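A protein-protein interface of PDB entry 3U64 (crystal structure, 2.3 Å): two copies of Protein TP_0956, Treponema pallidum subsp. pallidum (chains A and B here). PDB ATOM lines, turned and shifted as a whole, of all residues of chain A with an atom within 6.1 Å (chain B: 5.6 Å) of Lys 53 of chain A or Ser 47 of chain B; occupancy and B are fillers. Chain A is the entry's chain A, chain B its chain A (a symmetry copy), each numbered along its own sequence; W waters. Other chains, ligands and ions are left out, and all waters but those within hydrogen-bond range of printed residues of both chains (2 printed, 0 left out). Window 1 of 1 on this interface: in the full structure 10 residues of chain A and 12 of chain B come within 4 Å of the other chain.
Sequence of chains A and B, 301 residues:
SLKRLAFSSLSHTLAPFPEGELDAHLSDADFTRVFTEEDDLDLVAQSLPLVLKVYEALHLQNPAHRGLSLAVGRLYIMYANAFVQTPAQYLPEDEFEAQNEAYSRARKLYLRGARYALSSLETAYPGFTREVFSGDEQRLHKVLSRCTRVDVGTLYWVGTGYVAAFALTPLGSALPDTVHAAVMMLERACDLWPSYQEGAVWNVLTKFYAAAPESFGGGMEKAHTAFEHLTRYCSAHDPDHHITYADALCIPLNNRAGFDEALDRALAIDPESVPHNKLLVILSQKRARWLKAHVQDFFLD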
ATOM      1  N   LEU A  48      -2.798  -8.620  27.450  1.00  0.00           N
ATOM      2  CA  LEU A  48      -2.762  -9.499  26.281  1.00  0.00           C
ATOM      3  C   LEU A  48      -1.448 -10.330  26.109  1.00  0.00           C
ATOM      4  O   LEU A  48      -1.501 -11.497  25.719  1.00  0.00           O
ATOM      5  CB  LEU A  48      -3.126  -8.738  25.001  1.00  0.00           C
ATOM      6  CG  LEU A  48      -4.624  -8.653  24.697  1.00  0.00           C
ATOM      7  CD1 LEU A  48      -4.873  -8.017  23.334  1.00  0.00           C
ATOM      8  CD2 LEU A  48      -5.257 -10.044  24.763  1.00  0.00           C
ATOM      9  N   PRO A  49      -0.279  -9.745  26.427  1.00  0.00           N
ATOM     10  CA  PRO A  49       0.953 -10.528  26.225  1.00  0.00           C
ATOM     11  C   PRO A  49       0.982 -11.938  26.859  1.00  0.00           C
ATOM     12  O   PRO A  49       1.302 -12.890  26.137  1.00  0.00           O
ATOM     13  CB  PRO A  49       2.046  -9.622  26.802  1.00  0.00           C
ATOM     14  CG  PRO A  49       1.494  -8.219  26.593  1.00  0.00           C
ATOM     15  CD  PRO A  49       0.013  -8.368  26.876  1.00  0.00           C
ATOM     16  N   LEU A  50       0.682 -12.097  28.147  1.00  0.00           N
ATOM     17  CA  LEU A  50       0.730 -13.450  28.722  1.00  0.00           C
ATOM     18  C   LEU A  50      -0.310 -14.348  28.080  1.00  0.00           C
ATOM     19  O   LEU A  50      -0.061 -15.525  27.860  1.00  0.00           O
ATOM     20  CB  LEU A  50       0.583 -13.451  30.244  1.00  0.00           C
ATOM     21  CG  LEU A  50       0.685 -14.802  30.968  1.00  0.00           C
ATOM     22  CD1 LEU A  50       1.925 -15.646  30.558  1.00  0.00           C
ATOM     23  CD2 LEU A  50       0.674 -14.571  32.474  1.00  0.00           C
ATOM     24  N   VAL A  51      -1.471 -13.786  27.761  1.00  0.00           N
ATOM     25  CA  VAL A  51      -2.498 -14.511  27.009  1.00  0.00           C
ATOM     26  C   VAL A  51      -1.957 -15.065  25.678  1.00  0.00           C
ATOM     27  O   VAL A  51      -2.154 -16.241  25.345  1.00  0.00           O
ATOM     28  CB  VAL A  51      -3.701 -13.597  26.744  1.00  0.00           C
ATOM     29  CG1 VAL A  51      -4.723 -14.289  25.870  1.00  0.00           C
ATOM     30  CG2 VAL A  51      -4.326 -13.176  28.079  1.00  0.00           C
ATOM     31  N   LEU A  52      -1.284 -14.216  24.913  1.00  0.00           N
ATOM     32  CA  LEU A  52      -0.645 -14.672  23.690  1.00  0.00           C
ATOM     33  C   LEU A  52       0.288 -15.840  24.023  1.00  0.00           C
ATOM     34  O   LEU A  52       0.287 -16.874  23.353  1.00  0.00           O
ATOM     35  CB  LEU A  52       0.127 -13.534  23.031  1.00  0.00           C
ATOM     36  CG  LEU A  52      -0.534 -12.661  21.954  1.00  0.00           C
ATOM     37  CD1 LEU A  52      -1.968 -12.407  22.268  1.00  0.00           C
ATOM     38  CD2 LEU A  52       0.209 -11.339  21.827  1.00  0.00           C
ATOM     39  N   LYS A  53       1.061 -15.693  25.088  1.00  0.00           N
ATOM     40  CA  LYS A  53       2.037 -16.708  25.442  1.00  0.00           C
ATOM     41  C   LYS A  53       1.377 -18.028  25.837  1.00  0.00           C
ATOM     42  O   LYS A  53       1.832 -19.097  25.432  1.00  0.00           O
ATOM     43  CB  LYS A  53       2.981 -16.183  26.515  1.00  0.00           C
ATOM     44  CG  LYS A  53       3.955 -15.126  25.984  1.00  0.00           C
ATOM     45  CD  LYS A  53       5.118 -15.818  25.311  1.00  0.00           C
ATOM     46  CE  LYS A  53       5.376 -15.272  23.929  1.00  0.00           C
ATOM     47  NZ  LYS A  53       6.136 -16.284  23.114  1.00  0.00           N
ATOM     48  N   VAL A  54       0.286 -17.957  26.594  1.00  0.00           N
ATOM     49  CA  VAL A  54      -0.436 -19.171  26.973  1.00  0.00           C
ATOM     50  C   VAL A  54      -1.043 -19.881  25.769  1.00  0.00           C
ATOM     51  O   VAL A  54      -0.914 -21.100  25.629  1.00  0.00           O
ATOM     52  CB  VAL A  54      -1.515 -18.893  28.031  1.00  0.00           C
ATOM     53  CG1 VAL A  54      -2.415 -20.101  28.198  1.00  0.00           C
ATOM     54  CG2 VAL A  54      -0.849 -18.534  29.371  1.00  0.00           C
ATOM     55  N   TYR A  55      -1.693 -19.132  24.884  1.00  0.00           N
ATOM     56  CA  TYR A  55      -2.263 -19.760  23.698  1.00  0.00           C
ATOM     57  C   TYR A  55      -1.158 -20.371  22.870  1.00  0.00           C
ATOM     58  O   TYR A  55      -1.293 -21.465  22.327  1.00  0.00           O
ATOM     59  CB  TYR A  55      -3.019 -18.750  22.843  1.00  0.00           C
ATOM     60  CG  TYR A  55      -4.455 -18.568  23.259  1.00  0.00           C
ATOM     61  CD1 TYR A  55      -4.800 -17.692  24.286  1.00  0.00           C
ATOM     62  CD2 TYR A  55      -5.471 -19.259  22.621  1.00  0.00           C
ATOM     63  CE1 TYR A  55      -6.130 -17.516  24.667  1.00  0.00           C
ATOM     64  CE2 TYR A  55      -6.804 -19.089  22.992  1.00  0.00           C
ATOM     65  CZ  TYR A  55      -7.125 -18.216  24.012  1.00  0.00           C
ATOM     66  OH  TYR A  55      -8.447 -18.052  24.372  1.00  0.00           O
ATOM     67  N   GLU A  56      -0.055 -19.646  22.772  1.00  0.00           N
ATOM     68  CA  GLU A  56       1.052 -20.105  21.982  1.00  0.00           C
ATOM     69  C   GLU A  56       1.532 -21.439  22.529  1.00  0.00           C
ATOM     70  O   GLU A  56       1.776 -22.366  21.761  1.00  0.00           O
ATOM     71  CB  GLU A  56       2.168 -19.065  21.983  1.00  0.00           C
ATOM     72  CG  GLU A  56       3.122 -19.157  20.827  1.00  0.00           C
ATOM     73  CD  GLU A  56       4.073 -17.963  20.797  1.00  0.00           C
ATOM     74  OE1 GLU A  56       3.968 -17.125  21.712  1.00  0.00           O
ATOM     75  OE2 GLU A  56       4.909 -17.851  19.872  1.00  0.00           O
ATOM     76  N   ALA A  57       1.663 -21.541  23.853  1.00  0.00           N
ATOM     77  CA  ALA A  57       2.122 -22.786  24.468  1.00  0.00           C
ATOM     78  C   ALA A  57       1.107 -23.932  24.260  1.00  0.00           C
ATOM     79  O   ALA A  57       1.481 -25.070  23.970  1.00  0.00           O
ATOM     80  CB  ALA A  57       2.421 -22.582  25.957  1.00  0.00           C
ATOM     81  N   LEU A  58      -0.177 -23.622  24.398  1.00  0.00           N
ATOM     82  CA  LEU A  58      -1.212 -24.618  24.158  1.00  0.00           C
ATOM     83  C   LEU A  58      -1.119 -25.129  22.731  1.00  0.00           C
ATOM     84  O   LEU A  58      -1.236 -26.326  22.475  1.00  0.00           O
ATOM     85  CB  LEU A  58      -2.595 -24.030  24.414  1.00  0.00           C
ATOM     86  CG  LEU A  58      -2.893 -23.806  25.892  1.00  0.00           C
ATOM     87  CD1 LEU A  58      -4.309 -23.281  26.096  1.00  0.00           C
ATOM     88  CD2 LEU A  58      -2.686 -25.116  26.645  1.00  0.00           C
ATOM     89  N   TYR A  76      -2.086 -12.888  17.589  1.00  0.00           N
ATOM     90  CA  TYR A  76      -0.855 -12.188  17.227  1.00  0.00           C
ATOM     91  C   TYR A  76      -1.123 -11.080  16.221  1.00  0.00           C
ATOM     92  O   TYR A  76      -0.595  -9.973  16.363  1.00  0.00           O
ATOM     93  CB  TYR A  76       0.215 -13.153  16.710  1.00  0.00           C
ATOM     94  CG  TYR A  76       1.105 -13.632  17.834  1.00  0.00           C
ATOM     95  CD1 TYR A  76       0.908 -14.879  18.421  1.00  0.00           C
ATOM     96  CD2 TYR A  76       2.094 -12.805  18.357  1.00  0.00           C
ATOM     97  CE1 TYR A  76       1.698 -15.308  19.473  1.00  0.00           C
ATOM     98  CE2 TYR A  76       2.891 -13.215  19.419  1.00  0.00           C
ATOM     99  CZ  TYR A  76       2.686 -14.475  19.972  1.00  0.00           C
ATOM    100  OH  TYR A  76       3.456 -14.903  21.029  1.00  0.00           O
ATOM    101  N   ARG A 112       4.399 -14.061  12.179  1.00  0.00           N
ATOM    102  CA  ARG A 112       4.309 -15.171  13.130  1.00  0.00           C
ATOM    103  C   ARG A 112       2.846 -15.578  13.241  1.00  0.00           C
ATOM    104  O   ARG A 112       2.524 -16.766  13.251  1.00  0.00           O
ATOM    105  CB  ARG A 112       4.872 -14.782  14.506  1.00  0.00           C
ATOM    106  CG  ARG A 112       4.785 -15.885  15.580  1.00  0.00           C
ATOM    107  CD  ARG A 112       5.039 -15.344  16.991  1.00  0.00           C
ATOM    108  NE  ARG A 112       6.364 -14.735  17.101  1.00  0.00           N
ATOM    109  CZ  ARG A 112       6.887 -14.247  18.224  1.00  0.00           C
ATOM    110  NH1 ARG A 112       6.212 -14.291  19.359  1.00  0.00           N
ATOM    111  NH2 ARG A 112       8.094 -13.710  18.209  1.00  0.00           N
ATOM    112  N   PHE B  31       6.106 -25.005  28.664  1.00  0.00           N
ATOM    113  CA  PHE B  31       5.620 -23.635  28.693  1.00  0.00           C
ATOM    114  C   PHE B  31       6.817 -22.685  28.642  1.00  0.00           C
ATOM    115  O   PHE B  31       6.714 -21.530  28.208  1.00  0.00           O
ATOM    116  CB  PHE B  31       4.827 -23.453  29.998  1.00  0.00           C
ATOM    117  CG  PHE B  31       4.368 -22.038  30.278  1.00  0.00           C
ATOM    118  CD1 PHE B  31       3.658 -21.316  29.332  1.00  0.00           C
ATOM    119  CD2 PHE B  31       4.597 -21.459  31.524  1.00  0.00           C
ATOM    120  CE1 PHE B  31       3.211 -20.020  29.604  1.00  0.00           C
ATOM    121  CE2 PHE B  31       4.156 -20.164  31.811  1.00  0.00           C
ATOM    122  CZ  PHE B  31       3.461 -19.443  30.846  1.00  0.00           C
ATOM    123  N   VAL B  34       8.099 -21.315  25.011  1.00  0.00           N
ATOM    124  CA  VAL B  34       7.533 -20.097  24.443  1.00  0.00           C
ATOM    125  C   VAL B  34       8.208 -18.834  24.939  1.00  0.00           C
ATOM    126  O   VAL B  34       8.107 -17.792  24.297  1.00  0.00           O
ATOM    127  CB  VAL B  34       5.996 -20.013  24.601  1.00  0.00           C
ATOM    128  CG1 VAL B  34       5.351 -21.205  23.917  1.00  0.00           C
ATOM    129  CG2 VAL B  34       5.586 -19.941  26.057  1.00  0.00           C
ATOM    130  N   PHE B  35       8.908 -18.923  26.071  1.00  0.00           N
ATOM    131  CA  PHE B  35       9.696 -17.793  26.549  1.00  0.00           C
ATOM    132  C   PHE B  35      11.139 -17.877  26.060  1.00  0.00           C
ATOM    133  O   PHE B  35      11.661 -16.898  25.542  1.00  0.00           O
ATOM    134  CB  PHE B  35       9.623 -17.639  28.080  1.00  0.00           C
ATOM    135  CG  PHE B  35       8.244 -17.300  28.578  1.00  0.00           C
ATOM    136  CD1 PHE B  35       7.833 -15.984  28.687  1.00  0.00           C
ATOM    137  CD2 PHE B  35       7.342 -18.299  28.897  1.00  0.00           C
ATOM    138  CE1 PHE B  35       6.545 -15.670  29.111  1.00  0.00           C
ATOM    139  CE2 PHE B  35       6.057 -17.985  29.332  1.00  0.00           C
ATOM    140  CZ  PHE B  35       5.662 -16.676  29.435  1.00  0.00           C
ATOM    141  N   GLU B  38      11.777 -17.123  22.346  1.00  0.00           N
ATOM    142  CA  GLU B  38      11.202 -15.852  21.934  1.00  0.00           C
ATOM    143  C   GLU B  38      12.309 -14.960  21.344  1.00  0.00           C
ATOM    144  O   GLU B  38      13.476 -15.057  21.751  1.00  0.00           O
ATOM    145  CB  GLU B  38      10.507 -15.213  23.147  1.00  0.00           C
ATOM    146  CG  GLU B  38       9.695 -13.960  22.895  1.00  0.00           C
ATOM    147  CD  GLU B  38       8.665 -14.128  21.810  1.00  0.00           C
ATOM    148  OE1 GLU B  38       7.505 -14.432  22.126  1.00  0.00           O
ATOM    149  OE2 GLU B  38       9.013 -13.947  20.635  1.00  0.00           O
ATOM    150  N   ASP B  42       9.963  -7.373  24.430  1.00  0.00           N
ATOM    151  CA  ASP B  42       8.838  -6.698  25.075  1.00  0.00           C
ATOM    152  C   ASP B  42       7.722  -7.660  25.479  1.00  0.00           C
ATOM    153  O   ASP B  42       7.151  -7.519  26.558  1.00  0.00           O
ATOM    154  CB  ASP B  42       8.295  -5.567  24.199  1.00  0.00           C
ATOM    155  CG  ASP B  42       9.258  -4.387  24.110  1.00  0.00           C
ATOM    156  OD1 ASP B  42      10.094  -4.236  25.025  1.00  0.00           O
ATOM    157  OD2 ASP B  42       9.183  -3.612  23.125  1.00  0.00           O
ATOM    158  N   LEU B  43       7.409  -8.630  24.624  1.00  0.00           N
ATOM    159  CA  LEU B  43       6.391  -9.625  24.962  1.00  0.00           C
ATOM    160  C   LEU B  43       6.784 -10.407  26.214  1.00  0.00           C
ATOM    161  O   LEU B  43       5.949 -10.686  27.073  1.00  0.00           O
ATOM    162  CB  LEU B  43       6.153 -10.604  23.803  1.00  0.00           C
ATOM    163  CG  LEU B  43       5.278 -10.076  22.669  1.00  0.00           C
ATOM    164  CD1 LEU B  43       5.279 -11.027  21.485  1.00  0.00           C
ATOM    165  CD2 LEU B  43       3.879  -9.850  23.184  1.00  0.00           C
ATOM    166  N   VAL B  44       8.060 -10.768  26.305  1.00  0.00           N
ATOM    167  CA  VAL B  44       8.555 -11.486  27.470  1.00  0.00           C
ATOM    168  C   VAL B  44       8.490 -10.587  28.717  1.00  0.00           C
ATOM    169  O   VAL B  44       7.890 -10.964  29.718  1.00  0.00           O
ATOM    170  CB  VAL B  44       9.952 -12.036  27.232  1.00  0.00           C
ATOM    171  CG1 VAL B  44      10.394 -12.849  28.411  1.00  0.00           C
ATOM    172  CG2 VAL B  44       9.942 -12.921  25.981  1.00  0.00           C
ATOM    173  N   ALA B  45       9.063  -9.384  28.626  1.00  0.00           N
ATOM    174  CA  ALA B  45       9.098  -8.453  29.737  1.00  0.00           C
ATOM    175  C   ALA B  45       7.709  -8.202  30.297  1.00  0.00           C
ATOM    176  O   ALA B  45       7.535  -8.090  31.506  1.00  0.00           O
ATOM    177  CB  ALA B  45       9.762  -7.121  29.309  1.00  0.00           C
ATOM    178  N   GLN B  46       6.717  -8.092  29.423  1.00  0.00           N
ATOM    179  CA  GLN B  46       5.364  -7.755  29.876  1.00  0.00           C
ATOM    180  C   GLN B  46       4.586  -8.946  30.421  1.00  0.00           C
ATOM    181  O   GLN B  46       3.652  -8.772  31.201  1.00  0.00           O
ATOM    182  CB  GLN B  46       4.566  -7.084  28.761  1.00  0.00           C
ATOM    183  CG  GLN B  46       5.184  -5.765  28.329  1.00  0.00           C
ATOM    184  CD  GLN B  46       4.321  -5.014  27.349  1.00  0.00           C
ATOM    185  OE1 GLN B  46       3.103  -4.924  27.519  1.00  0.00           O
ATOM    186  NE2 GLN B  46       4.943  -4.468  26.310  1.00  0.00           N
ATOM    187  N   SER B  47       4.969 -10.153  30.020  1.00  0.00           N
ATOM    188  CA  SER B  47       4.254 -11.338  30.488  1.00  0.00           C
ATOM    189  C   SER B  47       4.913 -12.009  31.681  1.00  0.00           C
ATOM    190  O   SER B  47       4.244 -12.678  32.452  1.00  0.00           O
ATOM    191  CB  SER B  47       4.009 -12.339  29.343  1.00  0.00           C
ATOM    192  OG  SER B  47       5.197 -12.623  28.639  1.00  0.00           O
ATOM    193  N   LEU B  48       6.214 -11.808  31.874  1.00  0.00           N
ATOM    194  CA  LEU B  48       6.906 -12.513  32.954  1.00  0.00           C
ATOM    195  C   LEU B  48       6.412 -12.176  34.399  1.00  0.00           C
ATOM    196  O   LEU B  48       6.324 -13.066  35.245  1.00  0.00           O
ATOM    197  CB  LEU B  48       8.428 -12.371  32.825  1.00  0.00           C
ATOM    198  CG  LEU B  48       9.104 -13.407  31.923  1.00  0.00           C
ATOM    199  CD1 LEU B  48      10.623 -13.279  31.982  1.00  0.00           C
ATOM    200  CD2 LEU B  48       8.670 -14.819  32.320  1.00  0.00           C
ATOM    201  N   PRO B  49       6.062 -10.906  34.671  1.00  0.00           N
ATOM    202  CA  PRO B  49       5.634 -10.597  36.047  1.00  0.00           C
ATOM    203  C   PRO B  49       4.521 -11.494  36.638  1.00  0.00           C
ATOM    204  O   PRO B  49       4.718 -12.003  37.747  1.00  0.00           O
ATOM    205  CB  PRO B  49       5.196  -9.130  35.959  1.00  0.00           C
ATOM    206  CG  PRO B  49       6.058  -8.567  34.839  1.00  0.00           C
ATOM    207  CD  PRO B  49       6.119  -9.694  33.829  1.00  0.00           C
ATOM    208  N   LEU B  50       3.391 -11.687  35.961  1.00  0.00           N
ATOM    209  CA  LEU B  50       2.347 -12.536  36.556  1.00  0.00           C
ATOM    210  C   LEU B  50       2.833 -13.966  36.703  1.00  0.00           C
ATOM    211  O   LEU B  50       2.515 -14.632  37.679  1.00  0.00           O
ATOM    212  CB  LEU B  50       1.031 -12.489  35.780  1.00  0.00           C
ATOM    213  CG  LEU B  50      -0.157 -13.283  36.343  1.00  0.00           C
ATOM    214  CD1 LEU B  50      -0.426 -13.032  37.853  1.00  0.00           C
ATOM    215  CD2 LEU B  50      -1.404 -12.978  35.523  1.00  0.00           C
ATOM    216  N   VAL B  51       3.622 -14.432  35.740  1.00  0.00           N
ATOM    217  CA  VAL B  51       4.269 -15.743  35.840  1.00  0.00           C
ATOM    218  C   VAL B  51       5.104 -15.879  37.126  1.00  0.00           C
ATOM    219  O   VAL B  51       4.998 -16.872  37.858  1.00  0.00           O
ATOM    220  CB  VAL B  51       5.156 -15.987  34.613  1.00  0.00           C
ATOM    221  CG1 VAL B  51       5.923 -17.284  34.750  1.00  0.00           C
ATOM    222  CG2 VAL B  51       4.287 -16.004  33.350  1.00  0.00           C
HETATM  223  O   HOH W   1       0.647  -9.986  30.157  1.00  0.00           O
HETATM  224  O   HOH W   2       7.874 -17.856  20.806  1.00  0.00           O
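The side-chain amino group (NZ) of Lys 53 of chain A is in hydrogen-bond range of the backbone carbonyl oxygen (O) of Val 34 of chain B (2.7 Å). NZ of Lys 53 of chain A is in salt-bridge range of OE1 of Glu 38 of chain B. The side-chain carboxylate of Glu 38 of chain B is in salt-bridge range of the guanidinium group of Arg 112 of chain A, 2.6 Å away.
OE1 of Glu 56 of chain A is in salt-bridge range of NZ of Lys 53 of chain A (2.7 Å). The side-chain carboxylate of Glu 56 of chain A sits close to the side-chain hydroxyl of Tyr 76 of chain A, 3.5 Å away. NH1 of Arg 112 of chain A lies within salt-bridge range of OE2 of Glu 56 of chain A (3.8 Å). NH1 of Arg 112 of chain A is in hydrogen-bond range of OH of Tyr 76 of chain A (3.3 Å). The backbone carbonyl oxygen of Leu 43 of chain B is in hydrogen-bond range of the side-chain hydroxyl of Ser 47 of chain B (2.6 Å). The backbone carbonyl oxygen of Val 44 of chain B lies within hydrogen-bond range of the side-chain hydroxyl of Ser 47 of chain B, at 3.3 Å.
Pro 49 of chain A touches Gln 46 of chain B. Ser 47 of chain B touches Pro 49 of chain A (CB to C, 3.9 Å). CA of Leu 50 of chain A touches CB of Ser 47 of chain B, 3.5 Å away. Leu 50 of chain B touches Leu 50 of chain A. Leu 50 of chain A touches Val 51 of chain B (CD1 to CG2, 3.7 Å). Lys 53 of chain A touches Phe 35 of chain B (CB to CZ, 3.99 Å). Ser 47 of chain B touches Lys 53 of chain A. Ala 57 of chain A touches Phe 31 of chain B. Ala 57 of chain A touches Val 34 of chain B. Leu 43 of chain B touches Tyr 76 of chain A.
Leu 52 of chain A touches none of the printed residues of chain B. Printed residues of chain B within 4 Å of Lys 53 of chain A: Val 34 (2.7 Å), Phe 35 (3.99 Å), Glu 38 (2.5 Å) and Ser 47 (3.9 Å). Of the printed residues of chain A, Phe 31 of chain B touches Ala 57 (3.8 Å). Of the printed residues of chain A, Ser 47 of chain B touches Pro 49, Leu 50 and Lys 53. Printed residues of chain A within 4 Å of Leu 50 of chain B: Leu 50. The nearest printed residue of chain B that does not touch Lys 53 of chain A is Phe 31 of chain B (4.5 Å). The nearest residue of chain A that does not touch Ser 47 of chain B is Val 51 of chain A (5.9 Å). The nearest printed residue of chain A that does not touch Val 51 of chain B is Lys 53 of chain A (7.0 Å).
Of the 13 printed residues of chain A, 6 touch a printed residue of chain B. Among the printed residues, 13 pairs touch across the chains.
Leu 50 of chain A touches its own counterpart, Leu 50 of chain B. Leu 50 of chain A touches Val 51 of chain B, but with the chains exchanged Val 51 of chain A does not touch Leu 50 of chain B (7.8 Å). Positions printed for both chains: 48, 49, 50 and 51. Of the 13 pairs that touch across the chains among the printed residues, 1 has its exchanged pair printed and touching as well.
Water W1 lies within hydrogen-bond range of N of Leu 50 of chain A and O of Gln 46 of chain B. Water W2 lies within hydrogen-bond range of OE2 of Glu 56 of chain A (3.1 Å), NZ of Lys 53 of chain A (3.3 Å) and O of Val 34 of chain B (3.5 Å).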
